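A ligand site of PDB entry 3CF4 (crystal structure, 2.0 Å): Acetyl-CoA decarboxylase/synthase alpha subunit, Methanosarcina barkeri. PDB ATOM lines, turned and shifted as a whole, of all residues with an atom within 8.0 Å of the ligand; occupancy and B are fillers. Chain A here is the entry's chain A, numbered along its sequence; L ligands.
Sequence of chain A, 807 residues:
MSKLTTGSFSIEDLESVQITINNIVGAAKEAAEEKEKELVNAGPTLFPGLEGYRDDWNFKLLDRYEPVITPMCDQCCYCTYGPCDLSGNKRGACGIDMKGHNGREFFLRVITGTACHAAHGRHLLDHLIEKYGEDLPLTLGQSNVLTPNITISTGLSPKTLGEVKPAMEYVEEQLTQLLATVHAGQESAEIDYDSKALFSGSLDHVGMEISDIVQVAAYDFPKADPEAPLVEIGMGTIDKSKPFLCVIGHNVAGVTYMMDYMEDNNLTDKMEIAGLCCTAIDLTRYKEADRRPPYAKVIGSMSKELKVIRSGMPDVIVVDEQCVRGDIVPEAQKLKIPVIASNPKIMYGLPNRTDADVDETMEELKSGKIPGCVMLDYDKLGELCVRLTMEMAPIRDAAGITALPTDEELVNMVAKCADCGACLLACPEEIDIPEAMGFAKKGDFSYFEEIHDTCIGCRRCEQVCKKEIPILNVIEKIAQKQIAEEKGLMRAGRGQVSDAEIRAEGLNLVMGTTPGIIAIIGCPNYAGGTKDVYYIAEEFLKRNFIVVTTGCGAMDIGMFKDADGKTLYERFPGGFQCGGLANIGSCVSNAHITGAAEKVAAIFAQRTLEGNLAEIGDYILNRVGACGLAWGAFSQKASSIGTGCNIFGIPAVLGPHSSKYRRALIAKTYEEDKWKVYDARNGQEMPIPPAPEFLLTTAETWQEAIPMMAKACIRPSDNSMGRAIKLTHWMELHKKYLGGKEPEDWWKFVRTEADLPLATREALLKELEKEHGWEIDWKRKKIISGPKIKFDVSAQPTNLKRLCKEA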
ATOM      1  N   GLN A  75      11.235  -2.821 -21.931  1.00  0.00           N
ATOM      2  CA  GLN A  75      10.309  -1.748 -21.584  1.00  0.00           C
ATOM      3  C   GLN A  75      10.976  -0.403 -21.308  1.00  0.00           C
ATOM      4  O   GLN A  75      12.203  -0.307 -21.254  1.00  0.00           O
ATOM      5  CB  GLN A  75       9.500  -2.168 -20.353  1.00  0.00           C
ATOM      6  CG  GLN A  75       8.789  -3.518 -20.518  1.00  0.00           C
ATOM      7  CD  GLN A  75       8.213  -4.058 -19.212  1.00  0.00           C
ATOM      8  OE1 GLN A  75       7.488  -5.037 -19.205  1.00  0.00           O
ATOM      9  NE2 GLN A  75       8.529  -3.393 -18.109  1.00  0.00           N
ATOM     10  N   CYS A  76      10.145   0.618 -21.170  1.00  0.00           N
ATOM     11  CA  CYS A  76      10.591   1.960 -20.813  1.00  0.00           C
ATOM     12  C   CYS A  76       9.638   2.392 -19.703  1.00  0.00           C
ATOM     13  O   CYS A  76       8.415   2.252 -19.836  1.00  0.00           O
ATOM     14  CB  CYS A  76      10.477   2.967 -21.965  1.00  0.00           C
ATOM     15  SG  CYS A  76      10.847   4.677 -21.404  1.00  0.00           S
ATOM     16  N   CYS A  77      10.207   2.906 -18.614  1.00  0.00           N
ATOM     17  CA  CYS A  77       9.435   3.333 -17.456  1.00  0.00           C
ATOM     18  C   CYS A  77       9.807   4.757 -17.055  1.00  0.00           C
ATOM     19  O   CYS A  77       9.905   5.080 -15.864  1.00  0.00           O
ATOM     20  CB  CYS A  77       9.722   2.384 -16.277  1.00  0.00           C
ATOM     21  SG  CYS A  77      11.474   2.277 -15.770  1.00  0.00           S
ATOM     22  N   TYR A  78       9.998   5.615 -18.056  1.00  0.00           N
ATOM     23  CA  TYR A  78      10.374   7.010 -17.854  1.00  0.00           C
ATOM     24  C   TYR A  78       9.256   7.916 -17.350  1.00  0.00           C
ATOM     25  O   TYR A  78       9.499   8.806 -16.533  1.00  0.00           O
ATOM     26  CB  TYR A  78      10.908   7.605 -19.166  1.00  0.00           C
ATOM     27  CG  TYR A  78      12.408   7.493 -19.393  1.00  0.00           C
ATOM     28  CD1 TYR A  78      13.128   6.397 -18.947  1.00  0.00           C
ATOM     29  CD2 TYR A  78      13.071   8.464 -20.148  1.00  0.00           C
ATOM     30  CE1 TYR A  78      14.492   6.256 -19.255  1.00  0.00           C
ATOM     31  CE2 TYR A  78      14.420   8.342 -20.461  1.00  0.00           C
ATOM     32  CZ  TYR A  78      15.120   7.233 -20.024  1.00  0.00           C
ATOM     33  OH  TYR A  78      16.447   7.101 -20.355  1.00  0.00           O
ATOM     34  N   CYS A  79       8.033   7.699 -17.841  1.00  0.00           N
ATOM     35  CA  CYS A  79       6.935   8.588 -17.455  1.00  0.00           C
ATOM     36  C   CYS A  79       5.603   7.894 -17.147  1.00  0.00           C
ATOM     37  O   CYS A  79       5.469   6.679 -17.329  1.00  0.00           O
ATOM     38  CB  CYS A  79       6.733   9.626 -18.556  1.00  0.00           C
ATOM     39  SG  CYS A  79       5.763   9.001 -19.985  1.00  0.00           S
ATOM     40  N   THR A  80       4.603   8.664 -16.723  1.00  0.00           N
ATOM     41  CA  THR A  80       3.310   8.083 -16.346  1.00  0.00           C
ATOM     42  C   THR A  80       2.409   7.535 -17.460  1.00  0.00           C
ATOM     43  O   THR A  80       1.388   6.897 -17.161  1.00  0.00           O
ATOM     44  CB  THR A  80       2.481   9.053 -15.446  1.00  0.00           C
ATOM     45  OG1 THR A  80       1.724   9.957 -16.257  1.00  0.00           O
ATOM     46  CG2 THR A  80       3.402   9.833 -14.530  1.00  0.00           C
ATOM     47  N   TYR A  81       2.751   7.788 -18.720  1.00  0.00           N
ATOM     48  CA  TYR A  81       1.961   7.229 -19.825  1.00  0.00           C
ATOM     49  C   TYR A  81       2.318   5.749 -19.844  1.00  0.00           C
ATOM     50  O   TYR A  81       1.528   4.897 -20.269  1.00  0.00           O
ATOM     51  CB  TYR A  81       2.365   7.802 -21.199  1.00  0.00           C
ATOM     52  CG  TYR A  81       1.912   9.208 -21.510  1.00  0.00           C
ATOM     53  CD1 TYR A  81       2.819  10.166 -21.942  1.00  0.00           C
ATOM     54  CD2 TYR A  81       0.569   9.581 -21.402  1.00  0.00           C
ATOM     55  CE1 TYR A  81       2.417  11.468 -22.256  1.00  0.00           C
ATOM     56  CE2 TYR A  81       0.144  10.882 -21.711  1.00  0.00           C
ATOM     57  CZ  TYR A  81       1.075  11.817 -22.141  1.00  0.00           C
ATOM     58  OH  TYR A  81       0.697  13.116 -22.397  1.00  0.00           O
ATOM     59  N   GLY A  82       3.541   5.451 -19.388  1.00  0.00           N
ATOM     60  CA  GLY A  82       4.025   4.073 -19.376  1.00  0.00           C
ATOM     61  C   GLY A  82       3.718   3.254 -18.133  1.00  0.00           C
ATOM     62  O   GLY A  82       2.806   3.599 -17.380  1.00  0.00           O
ATOM     63  N   PRO A  83       4.470   2.159 -17.888  1.00  0.00           N
ATOM     64  CA  PRO A  83       5.562   1.671 -18.734  1.00  0.00           C
ATOM     65  C   PRO A  83       5.080   1.246 -20.114  1.00  0.00           C
ATOM     66  O   PRO A  83       3.905   0.927 -20.299  1.00  0.00           O
ATOM     67  CB  PRO A  83       6.101   0.463 -17.962  1.00  0.00           C
ATOM     68  CG  PRO A  83       5.607   0.663 -16.565  1.00  0.00           C
ATOM     69  CD  PRO A  83       4.246   1.256 -16.743  1.00  0.00           C
ATOM     70  N   CYS A  84       5.977   1.253 -21.086  1.00  0.00           N
ATOM     71  CA  CYS A  84       5.636   0.846 -22.438  1.00  0.00           C
ATOM     72  C   CYS A  84       6.413  -0.383 -22.891  1.00  0.00           C
ATOM     73  O   CYS A  84       7.634  -0.457 -22.703  1.00  0.00           O
ATOM     74  CB  CYS A  84       5.908   1.976 -23.430  1.00  0.00           C
ATOM     75  SG  CYS A  84       4.899   3.451 -23.119  1.00  0.00           S
ATOM     76  N   ASP A  85       5.724  -1.348 -23.462  1.00  0.00           N
ATOM     77  CA  ASP A  85       6.390  -2.519 -23.969  1.00  0.00           C
ATOM     78  C   ASP A  85       6.922  -2.145 -25.350  1.00  0.00           C
ATOM     79  O   ASP A  85       6.152  -1.902 -26.275  1.00  0.00           O
ATOM     80  CB  ASP A  85       5.429  -3.699 -24.098  1.00  0.00           C
ATOM     81  CG  ASP A  85       6.093  -4.898 -24.741  1.00  0.00           C
ATOM     82  OD1 ASP A  85       7.224  -5.249 -24.316  1.00  0.00           O
ATOM     83  OD2 ASP A  85       5.494  -5.493 -25.650  1.00  0.00           O
ATOM     84  N   LEU A  86       8.249  -2.105 -25.474  1.00  0.00           N
ATOM     85  CA  LEU A  86       8.889  -1.756 -26.735  1.00  0.00           C
ATOM     86  C   LEU A  86       9.385  -2.965 -27.533  1.00  0.00           C
ATOM     87  O   LEU A  86      10.001  -2.813 -28.589  1.00  0.00           O
ATOM     88  CB  LEU A  86      10.053  -0.796 -26.456  1.00  0.00           C
ATOM     89  CG  LEU A  86       9.641   0.508 -25.743  1.00  0.00           C
ATOM     90  CD1 LEU A  86      10.880   1.338 -25.402  1.00  0.00           C
ATOM     91  CD2 LEU A  86       8.687   1.291 -26.647  1.00  0.00           C
ATOM     92  N   LYS A  90       8.736  -1.793 -31.097  1.00  0.00           N
ATOM     93  CA  LYS A  90       7.449  -1.086 -31.110  1.00  0.00           C
ATOM     94  C   LYS A  90       7.757   0.297 -30.559  1.00  0.00           C
ATOM     95  O   LYS A  90       8.866   0.548 -30.043  1.00  0.00           O
ATOM     96  CB  LYS A  90       6.421  -1.764 -30.199  1.00  0.00           C
ATOM     97  CG  LYS A  90       5.675  -2.945 -30.849  1.00  0.00           C
ATOM     98  CD  LYS A  90       4.410  -3.342 -30.075  1.00  0.00           C
ATOM     99  CE  LYS A  90       4.707  -3.779 -28.638  1.00  0.00           C
ATOM    100  NZ  LYS A  90       5.568  -4.990 -28.550  1.00  0.00           N
ATOM    101  N   ARG A  91       6.777   1.199 -30.644  1.00  0.00           N
ATOM    102  CA  ARG A  91       6.948   2.564 -30.152  1.00  0.00           C
ATOM    103  C   ARG A  91       6.177   2.761 -28.849  1.00  0.00           C
ATOM    104  O   ARG A  91       5.107   2.186 -28.646  1.00  0.00           O
ATOM    105  CB  ARG A  91       6.471   3.560 -31.219  1.00  0.00           C
ATOM    106  CG  ARG A  91       7.351   3.564 -32.485  1.00  0.00           C
ATOM    107  CD  ARG A  91       6.811   4.492 -33.580  1.00  0.00           C
ATOM    108  NE  ARG A  91       7.689   4.516 -34.751  1.00  0.00           N
ATOM    109  CZ  ARG A  91       8.681   5.389 -34.944  1.00  0.00           C
ATOM    110  NH1 ARG A  91       8.949   6.332 -34.042  1.00  0.00           N
ATOM    111  NH2 ARG A  91       9.399   5.335 -36.055  1.00  0.00           N
ATOM    112  N   GLY A  92       6.731   3.582 -27.975  1.00  0.00           N
ATOM    113  CA  GLY A  92       6.060   3.866 -26.720  1.00  0.00           C
ATOM    114  C   GLY A  92       4.841   4.738 -26.980  1.00  0.00           C
ATOM    115  O   GLY A  92       4.604   5.145 -28.114  1.00  0.00           O
ATOM    116  N   ALA A  93       4.084   5.028 -25.944  1.00  0.00           N
ATOM    117  CA  ALA A  93       2.896   5.857 -26.083  1.00  0.00           C
ATOM    118  C   ALA A  93       3.266   7.237 -26.619  1.00  0.00           C
ATOM    119  O   ALA A  93       2.467   7.878 -27.303  1.00  0.00           O
ATOM    120  CB  ALA A  93       2.203   5.980 -24.731  1.00  0.00           C
ATOM    121  N   CYS A  94       4.476   7.701 -26.310  1.00  0.00           N
ATOM    122  CA  CYS A  94       4.945   9.015 -26.729  1.00  0.00           C
ATOM    123  C   CYS A  94       5.431   9.034 -28.188  1.00  0.00           C
ATOM    124  O   CYS A  94       5.614  10.106 -28.771  1.00  0.00           O
ATOM    125  CB  CYS A  94       6.087   9.482 -25.823  1.00  0.00           C
ATOM    126  SG  CYS A  94       7.571   8.422 -25.922  1.00  0.00           S
ATOM    127  N   GLY A  95       5.653   7.843 -28.740  1.00  0.00           N
ATOM    128  CA  GLY A  95       6.115   7.748 -30.107  1.00  0.00           C
ATOM    129  C   GLY A  95       7.540   7.260 -30.347  1.00  0.00           C
ATOM    130  O   GLY A  95       7.875   6.884 -31.481  1.00  0.00           O
ATOM    131  N   ILE A  96       8.386   7.233 -29.316  1.00  0.00           N
ATOM    132  CA  ILE A  96       9.766   6.789 -29.502  1.00  0.00           C
ATOM    133  C   ILE A  96       9.842   5.265 -29.649  1.00  0.00           C
ATOM    134  O   ILE A  96       9.146   4.526 -28.940  1.00  0.00           O
ATOM    135  CB  ILE A  96      10.659   7.271 -28.333  1.00  0.00           C
ATOM    136  CG1 ILE A  96      12.130   6.998 -28.636  1.00  0.00           C
ATOM    137  CG2 ILE A  96      10.218   6.619 -27.045  1.00  0.00           C
ATOM    138  CD1 ILE A  96      13.088   7.540 -27.554  1.00  0.00           C
ATOM    139  N   ASP A  97      10.668   4.791 -30.588  1.00  0.00           N
ATOM    140  CA  ASP A  97      10.786   3.348 -30.773  1.00  0.00           C
ATOM    141  C   ASP A  97      11.859   2.762 -29.876  1.00  0.00           C
ATOM    142  O   ASP A  97      12.581   3.494 -29.207  1.00  0.00           O
ATOM    143  CB  ASP A  97      11.027   2.953 -32.251  1.00  0.00           C
ATOM    144  CG  ASP A  97      12.326   3.517 -32.846  1.00  0.00           C
ATOM    145  OD1 ASP A  97      13.317   3.719 -32.110  1.00  0.00           O
ATOM    146  OD2 ASP A  97      12.354   3.726 -34.085  1.00  0.00           O
ATOM    147  N   MET A  98      11.927   1.438 -29.853  1.00  0.00           N
ATOM    148  CA  MET A  98      12.887   0.721 -29.013  1.00  0.00           C
ATOM    149  C   MET A  98      14.322   1.158 -29.219  1.00  0.00           C
ATOM    150  O   MET A  98      15.061   1.367 -28.262  1.00  0.00           O
ATOM    151  CB  MET A  98      12.773  -0.783 -29.225  1.00  0.00           C
ATOM    152  CG  MET A  98      13.590  -1.601 -28.250  1.00  0.00           C
ATOM    153  SD  MET A  98      13.355  -3.368 -28.473  1.00  0.00           S
ATOM    154  CE  MET A  98      12.959  -3.855 -26.824  1.00  0.00           C
ATOM    155  N   HIS A 101      14.825   4.606 -27.723  1.00  0.00           N
ATOM    156  CA  HIS A 101      14.876   4.562 -26.263  1.00  0.00           C
ATOM    157  C   HIS A 101      16.192   4.002 -25.734  1.00  0.00           C
ATOM    158  O   HIS A 101      16.718   4.474 -24.735  1.00  0.00           O
ATOM    159  CB  HIS A 101      13.715   3.738 -25.695  1.00  0.00           C
ATOM    160  CG  HIS A 101      13.772   3.556 -24.212  1.00  0.00           C
ATOM    161  ND1 HIS A 101      13.796   4.623 -23.343  1.00  0.00           N
ATOM    162  CD2 HIS A 101      13.894   2.436 -23.455  1.00  0.00           C
ATOM    163  CE1 HIS A 101      13.921   4.168 -22.102  1.00  0.00           C
ATOM    164  NE2 HIS A 101      13.985   2.848 -22.149  1.00  0.00           N
ATOM    165  N   ARG A 104      18.656   6.445 -26.087  1.00  0.00           N
ATOM    166  CA  ARG A 104      18.405   7.386 -25.009  1.00  0.00           C
ATOM    167  C   ARG A 104      18.959   6.858 -23.692  1.00  0.00           C
ATOM    168  O   ARG A 104      19.533   7.605 -22.913  1.00  0.00           O
ATOM    169  CB  ARG A 104      16.894   7.653 -24.904  1.00  0.00           C
ATOM    170  CG  ARG A 104      16.518   8.622 -23.790  1.00  0.00           C
ATOM    171  CD  ARG A 104      15.062   9.081 -23.896  1.00  0.00           C
ATOM    172  NE  ARG A 104      14.115   7.973 -23.741  1.00  0.00           N
ATOM    173  CZ  ARG A 104      12.798   8.106 -23.883  1.00  0.00           C
ATOM    174  NH1 ARG A 104      12.265   9.293 -24.167  1.00  0.00           N
ATOM    175  NH2 ARG A 104      12.017   7.051 -23.763  1.00  0.00           N
ATOM    176  N   VAL A 182      16.974  14.044 -21.961  1.00  0.00           N
ATOM    177  CA  VAL A 182      16.585  12.721 -21.475  1.00  0.00           C
ATOM    178  C   VAL A 182      15.080  12.720 -21.180  1.00  0.00           C
ATOM    179  O   VAL A 182      14.451  11.667 -21.097  1.00  0.00           O
ATOM    180  CB  VAL A 182      17.341  12.360 -20.184  1.00  0.00           C
ATOM    181  CG1 VAL A 182      16.752  11.088 -19.542  1.00  0.00           C
ATOM    182  CG2 VAL A 182      18.815  12.142 -20.491  1.00  0.00           C
ATOM    183  N   HIS A 183      14.504  13.925 -21.024  1.00  0.00           N
ATOM    184  CA  HIS A 183      13.071  14.089 -20.721  1.00  0.00           C
ATOM    185  C   HIS A 183      12.204  13.490 -21.827  1.00  0.00           C
ATOM    186  O   HIS A 183      12.553  13.558 -23.009  1.00  0.00           O
ATOM    187  CB  HIS A 183      12.760  15.587 -20.595  1.00  0.00           C
ATOM    188  CG  HIS A 183      11.378  15.886 -20.079  1.00  0.00           C
ATOM    189  ND1 HIS A 183      10.249  15.721 -20.847  1.00  0.00           N
ATOM    190  CD2 HIS A 183      10.959  16.358 -18.877  1.00  0.00           C
ATOM    191  CE1 HIS A 183       9.186  16.088 -20.145  1.00  0.00           C
ATOM    192  NE2 HIS A 183       9.590  16.470 -18.951  1.00  0.00           N
ATOM    193  N   ALA A 184      11.080  12.879 -21.444  1.00  0.00           N
ATOM    194  CA  ALA A 184      10.179  12.294 -22.440  1.00  0.00           C
ATOM    195  C   ALA A 184       9.784  13.358 -23.451  1.00  0.00           C
ATOM    196  O   ALA A 184       9.622  14.537 -23.097  1.00  0.00           O
ATOM    197  CB  ALA A 184       8.931  11.746 -21.760  1.00  0.00           C
ATOM    198  N   GLY A 185       9.625  12.945 -24.705  1.00  0.00           N
ATOM    199  CA  GLY A 185       9.214  13.873 -25.740  1.00  0.00           C
ATOM    200  C   GLY A 185      10.308  14.795 -26.222  1.00  0.00           C
ATOM    201  O   GLY A 185      10.054  15.956 -26.580  1.00  0.00           O
ATOM    202  N   GLN A 186      11.538  14.319 -26.210  1.00  0.00           N
ATOM    203  CA  GLN A 186      12.639  15.136 -26.686  1.00  0.00           C
ATOM    204  C   GLN A 186      13.140  14.411 -27.925  1.00  0.00           C
ATOM    205  O   GLN A 186      12.368  14.172 -28.860  1.00  0.00           O
ATOM    206  CB  GLN A 186      13.708  15.274 -25.593  1.00  0.00           C
ATOM    207  CG  GLN A 186      13.256  16.178 -24.421  1.00  0.00           C
ATOM    208  CD  GLN A 186      13.469  17.661 -24.691  1.00  0.00           C
ATOM    209  OE1 GLN A 186      13.170  18.153 -25.783  1.00  0.00           O
ATOM    210  NE2 GLN A 186      13.995  18.391 -23.700  1.00  0.00           N
HETATM  211 FE1  LIG L   1       8.903   5.792 -21.983  1.00  0.00          FE
HETATM  212 FE2  LIG L   1       6.902   7.496 -21.287  1.00  0.00          FE
HETATM  213 FE3  LIG L   1       6.407   5.137 -22.625  1.00  0.00          FE
HETATM  214 FE4  LIG L   1       7.636   7.186 -23.950  1.00  0.00          FE
HETATM  215  S1  LIG L   1       5.470   7.163 -23.087  1.00  0.00           S
HETATM  216  S2  LIG L   1       8.209   4.973 -24.081  1.00  0.00           S
HETATM  217  S3  LIG L   1       8.929   8.074 -22.208  1.00  0.00           S
HETATM  218  S4  LIG L   1       7.226   5.341 -20.453  1.00  0.00           S
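The side-chain sulfur (SG) of Cys 79 sits close to the backbone NH (N) of Tyr 81 (3.5 Å). The backbone NH (N) of Cys 84 sits at hydrogen-bond distance from the backbone carbonyl oxygen (O) of Cys 76 (2.9 Å). SG of Cys 76 sits close to ND1 of His 101, at 3.5 Å. The side-chain sulfur (SG) of Cys 94 sits close to the backbone NH (N) of Ile 96 (3.7 Å). The backbone NH of Tyr 78 sits close to the side-chain sulfur of Cys 76 (3.6 Å). NH2 of Arg 104 sits close to SG of Cys 76 (3.5 Å). SG of Cys 84 sits close to N of Ala 93 (3.3 Å). A ring nitrogen (ND1) of His 101 sits at hydrogen-bond distance from the guanidinium group (NH2) of Arg 104 (3.0 Å).
An iron atom (FE4) of the ligand is bound by the side-chain sulfur of Cys 94, 2.3 Å away. The backbone NH of Cys 79 lies close to a sulfur (S4) of the ligand, at 3.6 Å. The backbone NH (N) of Cys 94 lies close to a sulfur (S1) of the ligand, 3.4 Å away. An iron atom (FE3) of the ligand is bound by the side-chain sulfur (SG) of Cys 84 (2.3 Å). FE1 of the ligand is bound by SG of Cys 76. The backbone NH (N) of Tyr 78 sits close to a sulfur (S4) of the ligand, 3.7 Å away. S3 of the ligand sits close to NH2 of Arg 104 (3.6 Å). SG of Cys 79 binds FE2 of the ligand.
Residues that only touch the ligand: Gly 92 (3.6 Å), Gly 82 (3.6 Å), Tyr 81 (3.7 Å), Ala 184 (3.7 Å), Ala 93 (3.8 Å) and Ile 96 (3.9 Å). 12 residues have an atom within 4 Å of the ligand: Cys 76, Tyr 78, Cys 79, Tyr 81, Gly 82, Cys 84, Gly 92, Ala 93, Cys 94, Ile 96, Arg 104 and Ala 184.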
